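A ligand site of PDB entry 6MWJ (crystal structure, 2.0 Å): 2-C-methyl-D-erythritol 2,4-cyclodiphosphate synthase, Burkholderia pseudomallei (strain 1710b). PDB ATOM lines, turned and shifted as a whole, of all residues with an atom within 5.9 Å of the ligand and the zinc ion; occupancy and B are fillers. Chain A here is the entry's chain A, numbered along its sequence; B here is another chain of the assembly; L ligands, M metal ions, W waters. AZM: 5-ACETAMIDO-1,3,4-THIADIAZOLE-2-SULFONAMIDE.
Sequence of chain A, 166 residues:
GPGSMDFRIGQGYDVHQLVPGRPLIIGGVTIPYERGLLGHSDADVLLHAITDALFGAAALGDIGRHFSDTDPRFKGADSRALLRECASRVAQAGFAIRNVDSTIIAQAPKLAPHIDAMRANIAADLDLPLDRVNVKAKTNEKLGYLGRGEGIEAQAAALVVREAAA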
ATOM      1  N   TYR A  13     -14.079 -18.146  29.708  1.00  0.00           N
ATOM      2  CA  TYR A  13     -14.732 -16.837  29.701  1.00  0.00           C
ATOM      3  C   TYR A  13     -16.230 -17.061  29.585  1.00  0.00           C
ATOM      4  O   TYR A  13     -16.671 -17.977  28.881  1.00  0.00           O
ATOM      5  CB  TYR A  13     -14.237 -15.957  28.527  1.00  0.00           C
ATOM      6  CG  TYR A  13     -15.070 -14.716  28.268  1.00  0.00           C
ATOM      7  CD1 TYR A  13     -14.791 -13.519  28.932  1.00  0.00           C
ATOM      8  CD2 TYR A  13     -16.127 -14.729  27.346  1.00  0.00           C
ATOM      9  CE1 TYR A  13     -15.545 -12.379  28.705  1.00  0.00           C
ATOM     10  CE2 TYR A  13     -16.897 -13.589  27.126  1.00  0.00           C
ATOM     11  CZ  TYR A  13     -16.583 -12.413  27.796  1.00  0.00           C
ATOM     12  OH  TYR A  13     -17.332 -11.274  27.582  1.00  0.00           O
ATOM     13  N   ASP A  14     -17.021 -16.239  30.275  1.00  0.00           N
ATOM     14  CA  ASP A  14     -18.461 -16.273  30.033  1.00  0.00           C
ATOM     15  C   ASP A  14     -19.075 -14.936  30.440  1.00  0.00           C
ATOM     16  O   ASP A  14     -18.526 -14.216  31.271  1.00  0.00           O
ATOM     17  CB  ASP A  14     -19.136 -17.430  30.787  1.00  0.00           C
ATOM     18  CG  ASP A  14     -20.468 -17.822  30.174  1.00  0.00           C
ATOM     19  OD1 ASP A  14     -20.639 -17.624  28.952  1.00  0.00           O
ATOM     20  OD2 ASP A  14     -21.349 -18.290  30.900  1.00  0.00           O
ATOM     21  N   VAL A  15     -20.227 -14.630  29.841  1.00  0.00           N
ATOM     22  CA  VAL A  15     -21.035 -13.458  30.189  1.00  0.00           C
ATOM     23  C   VAL A  15     -22.500 -13.815  29.975  1.00  0.00           C
ATOM     24  O   VAL A  15     -22.844 -14.578  29.070  1.00  0.00           O
ATOM     25  CB  VAL A  15     -20.622 -12.215  29.359  1.00  0.00           C
ATOM     26  CG1 VAL A  15     -21.026 -12.357  27.900  1.00  0.00           C
ATOM     27  CG2 VAL A  15     -21.219 -10.959  29.961  1.00  0.00           C
ATOM     28  N   HIS A  16     -23.373 -13.269  30.825  1.00  0.00           N
ATOM     29  CA  HIS A  16     -24.813 -13.392  30.614  1.00  0.00           C
ATOM     30  C   HIS A  16     -25.458 -12.070  30.963  1.00  0.00           C
ATOM     31  O   HIS A  16     -24.993 -11.358  31.863  1.00  0.00           O
ATOM     32  CB  HIS A  16     -25.447 -14.494  31.479  1.00  0.00           C
ATOM     33  CG  HIS A  16     -25.129 -15.877  31.001  1.00  0.00           C
ATOM     34  ND1 HIS A  16     -25.973 -16.585  30.165  1.00  0.00           N
ATOM     35  CD2 HIS A  16     -24.062 -16.682  31.248  1.00  0.00           C
ATOM     36  CE1 HIS A  16     -25.436 -17.775  29.917  1.00  0.00           C
ATOM     37  NE2 HIS A  16     -24.283 -17.860  30.559  1.00  0.00           N
ATOM     38  N   HIS A  40     -30.241 -20.280  28.626  1.00  0.00           N
ATOM     39  CA  HIS A  40     -31.006 -21.519  28.439  1.00  0.00           C
ATOM     40  C   HIS A  40     -30.958 -22.384  29.693  1.00  0.00           C
ATOM     41  O   HIS A  40     -31.985 -22.881  30.163  1.00  0.00           O
ATOM     42  CB  HIS A  40     -30.461 -22.276  27.228  1.00  0.00           C
ATOM     43  CG  HIS A  40     -31.258 -23.494  26.862  1.00  0.00           C
ATOM     44  ND1 HIS A  40     -32.529 -23.422  26.334  1.00  0.00           N
ATOM     45  CD2 HIS A  40     -30.942 -24.810  26.936  1.00  0.00           C
ATOM     46  CE1 HIS A  40     -32.967 -24.657  26.099  1.00  0.00           C
ATOM     47  NE2 HIS A  40     -32.031 -25.504  26.457  1.00  0.00           N
ATOM     48  N   SER A  41     -29.761 -22.556  30.269  1.00  0.00           N
ATOM     49  CA  SER A  41     -29.608 -23.217  31.557  1.00  0.00           C
ATOM     50  C   SER A  41     -29.979 -22.252  32.676  1.00  0.00           C
ATOM     51  O   SER A  41     -30.641 -21.231  32.428  1.00  0.00           O
ATOM     52  CB  SER A  41     -28.173 -23.709  31.759  1.00  0.00           C
ATOM     53  OG  SER A  41     -27.260 -22.603  31.835  1.00  0.00           O
ATOM     54  N   ALA A  43     -27.922 -20.336  33.718  1.00  0.00           N
ATOM     55  CA  ALA A  43     -27.105 -19.188  33.319  1.00  0.00           C
ATOM     56  C   ALA A  43     -26.010 -18.861  34.339  1.00  0.00           C
ATOM     57  O   ALA A  43     -25.579 -17.697  34.423  1.00  0.00           O
ATOM     58  CB  ALA A  43     -27.965 -17.931  33.058  1.00  0.00           C
ATOM     59  N   ASP A  44     -25.538 -19.852  35.083  1.00  0.00           N
ATOM     60  CA  ASP A  44     -24.471 -19.656  36.065  1.00  0.00           C
ATOM     61  C   ASP A  44     -23.167 -19.297  35.377  1.00  0.00           C
ATOM     62  O   ASP A  44     -22.398 -20.194  34.979  1.00  0.00           O
ATOM     63  CB  ASP A  44     -24.324 -20.915  36.925  1.00  0.00           C
ATOM     64  CG  ASP A  44     -23.514 -20.677  38.185  1.00  0.00           C
ATOM     65  OD1 ASP A  44     -22.512 -19.937  38.115  1.00  0.00           O
ATOM     66  OD2 ASP A  44     -23.870 -21.248  39.246  1.00  0.00           O
ATOM     67  N   VAL A  45     -22.880 -18.001  35.258  1.00  0.00           N
ATOM     68  CA  VAL A  45     -21.767 -17.527  34.426  1.00  0.00           C
ATOM     69  C   VAL A  45     -20.421 -17.982  34.985  1.00  0.00           C
ATOM     70  O   VAL A  45     -19.493 -18.286  34.219  1.00  0.00           O
ATOM     71  CB  VAL A  45     -21.850 -15.987  34.281  1.00  0.00           C
ATOM     72  CG1 VAL A  45     -21.671 -15.301  35.638  1.00  0.00           C
ATOM     73  CG2 VAL A  45     -20.833 -15.477  33.271  1.00  0.00           C
ATOM     74  N   HIS A  48     -19.964 -21.810  34.181  1.00  0.00           N
ATOM     75  CA  HIS A  48     -19.733 -21.990  32.747  1.00  0.00           C
ATOM     76  C   HIS A  48     -18.301 -21.649  32.381  1.00  0.00           C
ATOM     77  O   HIS A  48     -17.659 -22.373  31.598  1.00  0.00           O
ATOM     78  CB  HIS A  48     -20.703 -21.122  31.938  1.00  0.00           C
ATOM     79  CG  HIS A  48     -22.140 -21.541  32.057  1.00  0.00           C
ATOM     80  ND1 HIS A  48     -23.150 -20.915  31.353  1.00  0.00           N
ATOM     81  CD2 HIS A  48     -22.731 -22.517  32.782  1.00  0.00           C
ATOM     82  CE1 HIS A  48     -24.297 -21.490  31.645  1.00  0.00           C
ATOM     83  NE2 HIS A  48     -24.075 -22.461  32.513  1.00  0.00           N
ATOM     84  N   ALA A  49     -17.770 -20.556  32.928  1.00  0.00           N
ATOM     85  CA  ALA A  49     -16.379 -20.191  32.684  1.00  0.00           C
ATOM     86  C   ALA A  49     -15.425 -21.270  33.192  1.00  0.00           C
ATOM     87  O   ALA A  49     -14.471 -21.646  32.501  1.00  0.00           O
ATOM     88  CB  ALA A  49     -16.068 -18.849  33.339  1.00  0.00           C
ATOM     89  N   ASP A  52     -15.599 -24.353  30.936  1.00  0.00           N
ATOM     90  CA  ASP A  52     -14.831 -24.145  29.715  1.00  0.00           C
ATOM     91  C   ASP A  52     -13.340 -24.308  29.961  1.00  0.00           C
ATOM     92  O   ASP A  52     -12.635 -24.900  29.138  1.00  0.00           O
ATOM     93  CB  ASP A  52     -15.110 -22.744  29.131  1.00  0.00           C
ATOM     94  CG  ASP A  52     -15.882 -22.788  27.825  1.00  0.00           C
ATOM     95  OD1 ASP A  52     -16.310 -23.894  27.418  1.00  0.00           O
ATOM     96  OD2 ASP A  52     -16.070 -21.710  27.201  1.00  0.00           O
ATOM     97  N   ILE A  63     -18.013 -26.039  26.427  1.00  0.00           N
ATOM     98  CA  ILE A  63     -19.242 -26.406  27.127  1.00  0.00           C
ATOM     99  C   ILE A  63     -20.386 -26.591  26.143  1.00  0.00           C
ATOM    100  O   ILE A  63     -21.222 -27.485  26.309  1.00  0.00           O
ATOM    101  CB  ILE A  63     -19.560 -25.341  28.192  1.00  0.00           C
ATOM    102  CG1 ILE A  63     -20.812 -25.726  28.979  1.00  0.00           C
ATOM    103  CG2 ILE A  63     -19.651 -23.920  27.564  1.00  0.00           C
ATOM    104  CD1 ILE A  63     -21.098 -24.808  30.180  1.00  0.00           C
ATOM    105  N   GLY A  64     -20.429 -25.790  25.075  1.00  0.00           N
ATOM    106  CA  GLY A  64     -21.471 -25.934  24.071  1.00  0.00           C
ATOM    107  C   GLY A  64     -21.381 -27.224  23.284  1.00  0.00           C
ATOM    108  O   GLY A  64     -22.402 -27.799  22.901  1.00  0.00           O
ATOM    109  N   ARG A  65     -20.157 -27.697  23.022  1.00  0.00           N
ATOM    110  CA  ARG A  65     -19.990 -29.012  22.416  1.00  0.00           C
ATOM    111  C   ARG A  65     -20.562 -30.112  23.308  1.00  0.00           C
ATOM    112  O   ARG A  65     -21.194 -31.049  22.823  1.00  0.00           O
ATOM    113  CB  ARG A  65     -18.511 -29.287  22.142  1.00  0.00           C
ATOM    114  CG  ARG A  65     -18.218 -30.744  21.824  1.00  0.00           C
ATOM    115  CD  ARG A  65     -16.772 -30.976  21.484  1.00  0.00           C
ATOM    116  NE  ARG A  65     -16.334 -32.309  21.868  1.00  0.00           N
ATOM    117  CZ  ARG A  65     -15.100 -32.776  21.673  1.00  0.00           C
ATOM    118  NH1 ARG A  65     -14.794 -34.017  22.056  1.00  0.00           N
ATOM    119  NH2 ARG A  65     -14.179 -31.998  21.090  1.00  0.00           N
ATOM    120  N   PHE A  67     -22.695 -29.811  26.124  1.00  0.00           N
ATOM    121  CA  PHE A  67     -24.063 -29.613  26.605  1.00  0.00           C
ATOM    122  C   PHE A  67     -24.724 -28.544  25.721  1.00  0.00           C
ATOM    123  O   PHE A  67     -24.552 -27.348  25.965  1.00  0.00           O
ATOM    124  CB  PHE A  67     -24.052 -29.194  28.076  1.00  0.00           C
ATOM    125  CG  PHE A  67     -23.081 -29.969  28.940  1.00  0.00           C
ATOM    126  CD1 PHE A  67     -23.307 -31.316  29.244  1.00  0.00           C
ATOM    127  CD2 PHE A  67     -21.964 -29.351  29.486  1.00  0.00           C
ATOM    128  CE1 PHE A  67     -22.433 -32.017  30.058  1.00  0.00           C
ATOM    129  CE2 PHE A  67     -21.090 -30.052  30.300  1.00  0.00           C
ATOM    130  CZ  PHE A  67     -21.325 -31.386  30.586  1.00  0.00           C
ATOM    131  N   SER A  68     -25.498 -28.980  24.723  1.00  0.00           N
ATOM    132  CA  SER A  68     -26.114 -28.072  23.763  1.00  0.00           C
ATOM    133  C   SER A  68     -26.945 -26.991  24.441  1.00  0.00           C
ATOM    134  O   SER A  68     -27.798 -27.289  25.279  1.00  0.00           O
ATOM    135  CB  SER A  68     -26.993 -28.865  22.795  1.00  0.00           C
ATOM    136  OG  SER A  68     -27.840 -28.005  22.031  1.00  0.00           O
ATOM    137  N   ASP A  69     -26.710 -25.735  24.061  1.00  0.00           N
ATOM    138  CA  ASP A  69     -27.416 -24.612  24.669  1.00  0.00           C
ATOM    139  C   ASP A  69     -28.795 -24.371  24.067  1.00  0.00           C
ATOM    140  O   ASP A  69     -29.442 -23.380  24.409  1.00  0.00           O
ATOM    141  CB  ASP A  69     -26.583 -23.326  24.565  1.00  0.00           C
ATOM    142  CG  ASP A  69     -26.722 -22.443  25.805  1.00  0.00           C
ATOM    143  OD1 ASP A  69     -27.056 -22.976  26.891  1.00  0.00           O
ATOM    144  OD2 ASP A  69     -26.500 -21.211  25.702  1.00  0.00           O
ATOM    145  N   PHE A  74     -31.884 -29.341  28.558  1.00  0.00           N
ATOM    146  CA  PHE A  74     -31.023 -28.492  29.383  1.00  0.00           C
ATOM    147  C   PHE A  74     -31.691 -27.177  29.750  1.00  0.00           C
ATOM    148  O   PHE A  74     -31.031 -26.291  30.303  1.00  0.00           O
ATOM    149  CB  PHE A  74     -29.694 -28.224  28.666  1.00  0.00           C
ATOM    150  CG  PHE A  74     -28.810 -29.438  28.538  1.00  0.00           C
ATOM    151  CD1 PHE A  74     -28.448 -30.186  29.660  1.00  0.00           C
ATOM    152  CD2 PHE A  74     -28.331 -29.839  27.297  1.00  0.00           C
ATOM    153  CE1 PHE A  74     -27.632 -31.298  29.533  1.00  0.00           C
ATOM    154  CE2 PHE A  74     -27.513 -30.954  27.161  1.00  0.00           C
ATOM    155  CZ  PHE A  74     -27.154 -31.675  28.295  1.00  0.00           C
ATOM    156  N   ALA A  77     -31.227 -26.072  33.224  1.00  0.00           N
ATOM    157  CA  ALA A  77     -30.281 -27.044  33.769  1.00  0.00           C
ATOM    158  C   ALA A  77     -29.472 -26.459  34.921  1.00  0.00           C
ATOM    159  O   ALA A  77     -29.071 -25.295  34.909  1.00  0.00           O
ATOM    160  CB  ALA A  77     -29.348 -27.540  32.678  1.00  0.00           C
ATOM    161  N   SER A  79     -26.292 -25.822  36.592  1.00  0.00           N
ATOM    162  CA  SER A  79     -24.928 -25.765  36.066  1.00  0.00           C
ATOM    163  C   SER A  79     -23.912 -26.456  36.957  1.00  0.00           C
ATOM    164  O   SER A  79     -22.780 -26.682  36.511  1.00  0.00           O
ATOM    165  CB  SER A  79     -24.507 -24.316  35.800  1.00  0.00           C
ATOM    166  OG  SER A  79     -25.203 -23.770  34.671  1.00  0.00           O
ATOM    167  N   LEU A  82     -23.814 -29.826  35.393  1.00  0.00           N
ATOM    168  CA  LEU A  82     -22.984 -29.758  34.192  1.00  0.00           C
ATOM    169  C   LEU A  82     -21.507 -29.736  34.556  1.00  0.00           C
ATOM    170  O   LEU A  82     -20.690 -30.423  33.914  1.00  0.00           O
ATOM    171  CB  LEU A  82     -23.350 -28.530  33.351  1.00  0.00           C
ATOM    172  CG  LEU A  82     -24.797 -28.381  32.849  1.00  0.00           C
ATOM    173  CD1 LEU A  82     -24.958 -27.088  32.006  1.00  0.00           C
ATOM    174  CD2 LEU A  82     -25.234 -29.603  32.044  1.00  0.00           C
ATOM    175  N   LYS B 138     -17.807 -18.934  21.428  1.00  0.00           N
ATOM    176  CA  LYS B 138     -19.093 -18.598  22.025  1.00  0.00           C
ATOM    177  C   LYS B 138     -19.455 -17.164  21.670  1.00  0.00           C
ATOM    178  O   LYS B 138     -18.592 -16.379  21.255  1.00  0.00           O
ATOM    179  CB  LYS B 138     -19.059 -18.767  23.539  1.00  0.00           C
ATOM    180  CG  LYS B 138     -18.058 -17.830  24.207  1.00  0.00           C
ATOM    181  CD  LYS B 138     -18.148 -17.910  25.723  1.00  0.00           C
ATOM    182  CE  LYS B 138     -18.015 -19.339  26.192  1.00  0.00           C
ATOM    183  NZ  LYS B 138     -18.484 -19.555  27.581  1.00  0.00           N
ATOM    184  N   THR B 139     -20.730 -16.818  21.842  1.00  0.00           N
ATOM    185  CA  THR B 139     -21.177 -15.454  21.597  1.00  0.00           C
ATOM    186  C   THR B 139     -20.928 -14.595  22.836  1.00  0.00           C
ATOM    187  O   THR B 139     -20.504 -15.073  23.893  1.00  0.00           O
ATOM    188  CB  THR B 139     -22.663 -15.423  21.234  1.00  0.00           C
ATOM    189  OG1 THR B 139     -23.448 -15.628  22.418  1.00  0.00           O
ATOM    190  CG2 THR B 139     -23.016 -16.521  20.223  1.00  0.00           C
ATOM    191  N   GLU B 141     -23.526 -12.867  24.087  1.00  0.00           N
ATOM    192  CA  GLU B 141     -24.890 -12.667  24.590  1.00  0.00           C
ATOM    193  C   GLU B 141     -25.424 -11.281  24.239  1.00  0.00           C
ATOM    194  O   GLU B 141     -26.139 -10.656  25.015  1.00  0.00           O
ATOM    195  CB  GLU B 141     -24.967 -12.910  26.100  1.00  0.00           C
ATOM    196  CG  GLU B 141     -24.661 -14.328  26.490  1.00  0.00           C
ATOM    197  CD  GLU B 141     -25.673 -15.284  25.935  1.00  0.00           C
ATOM    198  OE1 GLU B 141     -26.886 -15.029  26.078  1.00  0.00           O
ATOM    199  OE2 GLU B 141     -25.249 -16.293  25.334  1.00  0.00           O
HETATM  200  C1  AZM L   1     -22.829 -22.141  27.243  1.00  0.00           C
HETATM  201  C2  AZM L   1     -24.076 -24.171  27.287  1.00  0.00           C
HETATM  202  C3  AZM L   1     -25.719 -25.321  28.735  1.00  0.00           C
HETATM  203  C4  AZM L   1     -26.526 -26.602  28.703  1.00  0.00           C
HETATM  204  N1  AZM L   1     -21.788 -19.944  26.075  1.00  0.00           N
HETATM  205  N2  AZM L   1     -23.404 -24.034  26.196  1.00  0.00           N
HETATM  206  N3  AZM L   1     -22.655 -22.818  26.202  1.00  0.00           N
HETATM  207  N4  AZM L   1     -24.907 -25.198  27.587  1.00  0.00           N
HETATM  208  O1  AZM L   1     -23.170 -19.725  28.297  1.00  0.00           O
HETATM  209  O2  AZM L   1     -20.693 -20.850  28.376  1.00  0.00           O
HETATM  210  O3  AZM L   1     -25.759 -24.507  29.611  1.00  0.00           O
HETATM  211  S1  AZM L   1     -22.038 -20.587  27.612  1.00  0.00           S
HETATM  212  S2  AZM L   1     -23.913 -22.816  28.487  1.00  0.00           S
HETATM  213 ZN    ZN M   1     -22.970 -19.187  30.200  1.00  0.00          ZN
HETATM  214  O   HOH W   1     -27.136 -21.337  29.345  1.00  0.00           O
HETATM  215  O   HOH W   2     -22.407 -19.224  22.992  1.00  0.00           O
HETATM  216  O   HOH W   3     -20.221 -22.857  24.256  1.00  0.00           O
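Residues that only touch the ligand: Ile 63 (3.3 Å), Gly 64 (3.4 Å), Ser 68 (3.7 Å), Phe 74 (3.6 Å) and Leu 82 (3.6 Å).
Hydrophobic or aromatic side chains that line the ligand: His 16, His 48, Ile 63, Phe 67, Phe 74 and Leu 82.
Within 4 Å of the ligand: Asp 14, His 16, Ser 41, His 48, Ile 63, Gly 64, Phe 67, Ser 68, Asp 69, Phe 74, Leu 82 and Lys 138 of chain B.
The nearest printed residue that does not touch the ligand is Asp 52 (4.8 Å).
Water W3 lies within hydrogen-bond range of N of Gly 64 (3.1 Å) and N3 of the ligand (3.1 Å).
Water W2 bridges the backbone NH of Thr 139 of chain B and a nitrogen (N1) of the ligand.
Water W1 lies within hydrogen-bond range of OG of Ser 41 (2.8 Å), OD1 of Asp 69 (3.0 Å), N of His 40 (3.4 Å) and O3 of the ligand (3.5 Å).
A ring nitrogen (NE2) of His 16 binds the zinc ion (1.9 Å).
The zinc ion is bound by the side-chain carboxylate (OD2) of Asp 14, at 2.0 Å.
The zinc ion is bound by O1 of the ligand, 2.0 Å away.
ND1 of His 48 binds the zinc ion.
The side-chain carboxylate (OD1) of Asp 14 is in salt-bridge range of the side-chain amino group (NZ) of Lys 138 of chain B (3.2 Å).
OG of Ser 41 lies close to NE2 of His 48, 3.3 Å away.
The side-chain hydroxyl of Ser 79 lies within hydrogen-bond range of a ring nitrogen (NE2) of His 48, at 2.8 Å.
The side-chain amino group of Lys 138 of chain B is in salt-bridge range of the side-chain carboxylate of Asp 52.
The side-chain amino group of Lys 138 of chain B sits at hydrogen-bond distance from the backbone carbonyl oxygen of Tyr 13 (2.7 Å).
OG of Ser 41 lies close to N of Ala 43.
The backbone NH (N) of Ile 63 is in hydrogen-bond range of the side-chain carboxylate (OD1) of Asp 52, 2.9 Å away.
Within 4 Å of the zinc ion: Asp 14, His 16 and His 48.
The nearest printed residue that does not touch the zinc ion is Val 45 (4.7 Å).
The side-chain amino group (NZ) of Lys 138 of chain B lies within hydrogen-bond range of an oxygen (O2) of the ligand.
A nitrogen (N4) of the ligand sits at hydrogen-bond distance from the backbone carbonyl oxygen (O) of Phe 67 (2.7 Å).
The side-chain carboxylate (OD1) of Asp 69 sits at hydrogen-bond distance from a nitrogen (N4) of the ligand, at 3.2 Å.
The side-chain hydroxyl (OG) of Ser 41 is in hydrogen-bond range of an oxygen (O3) of the ligand, 3.3 Å away.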
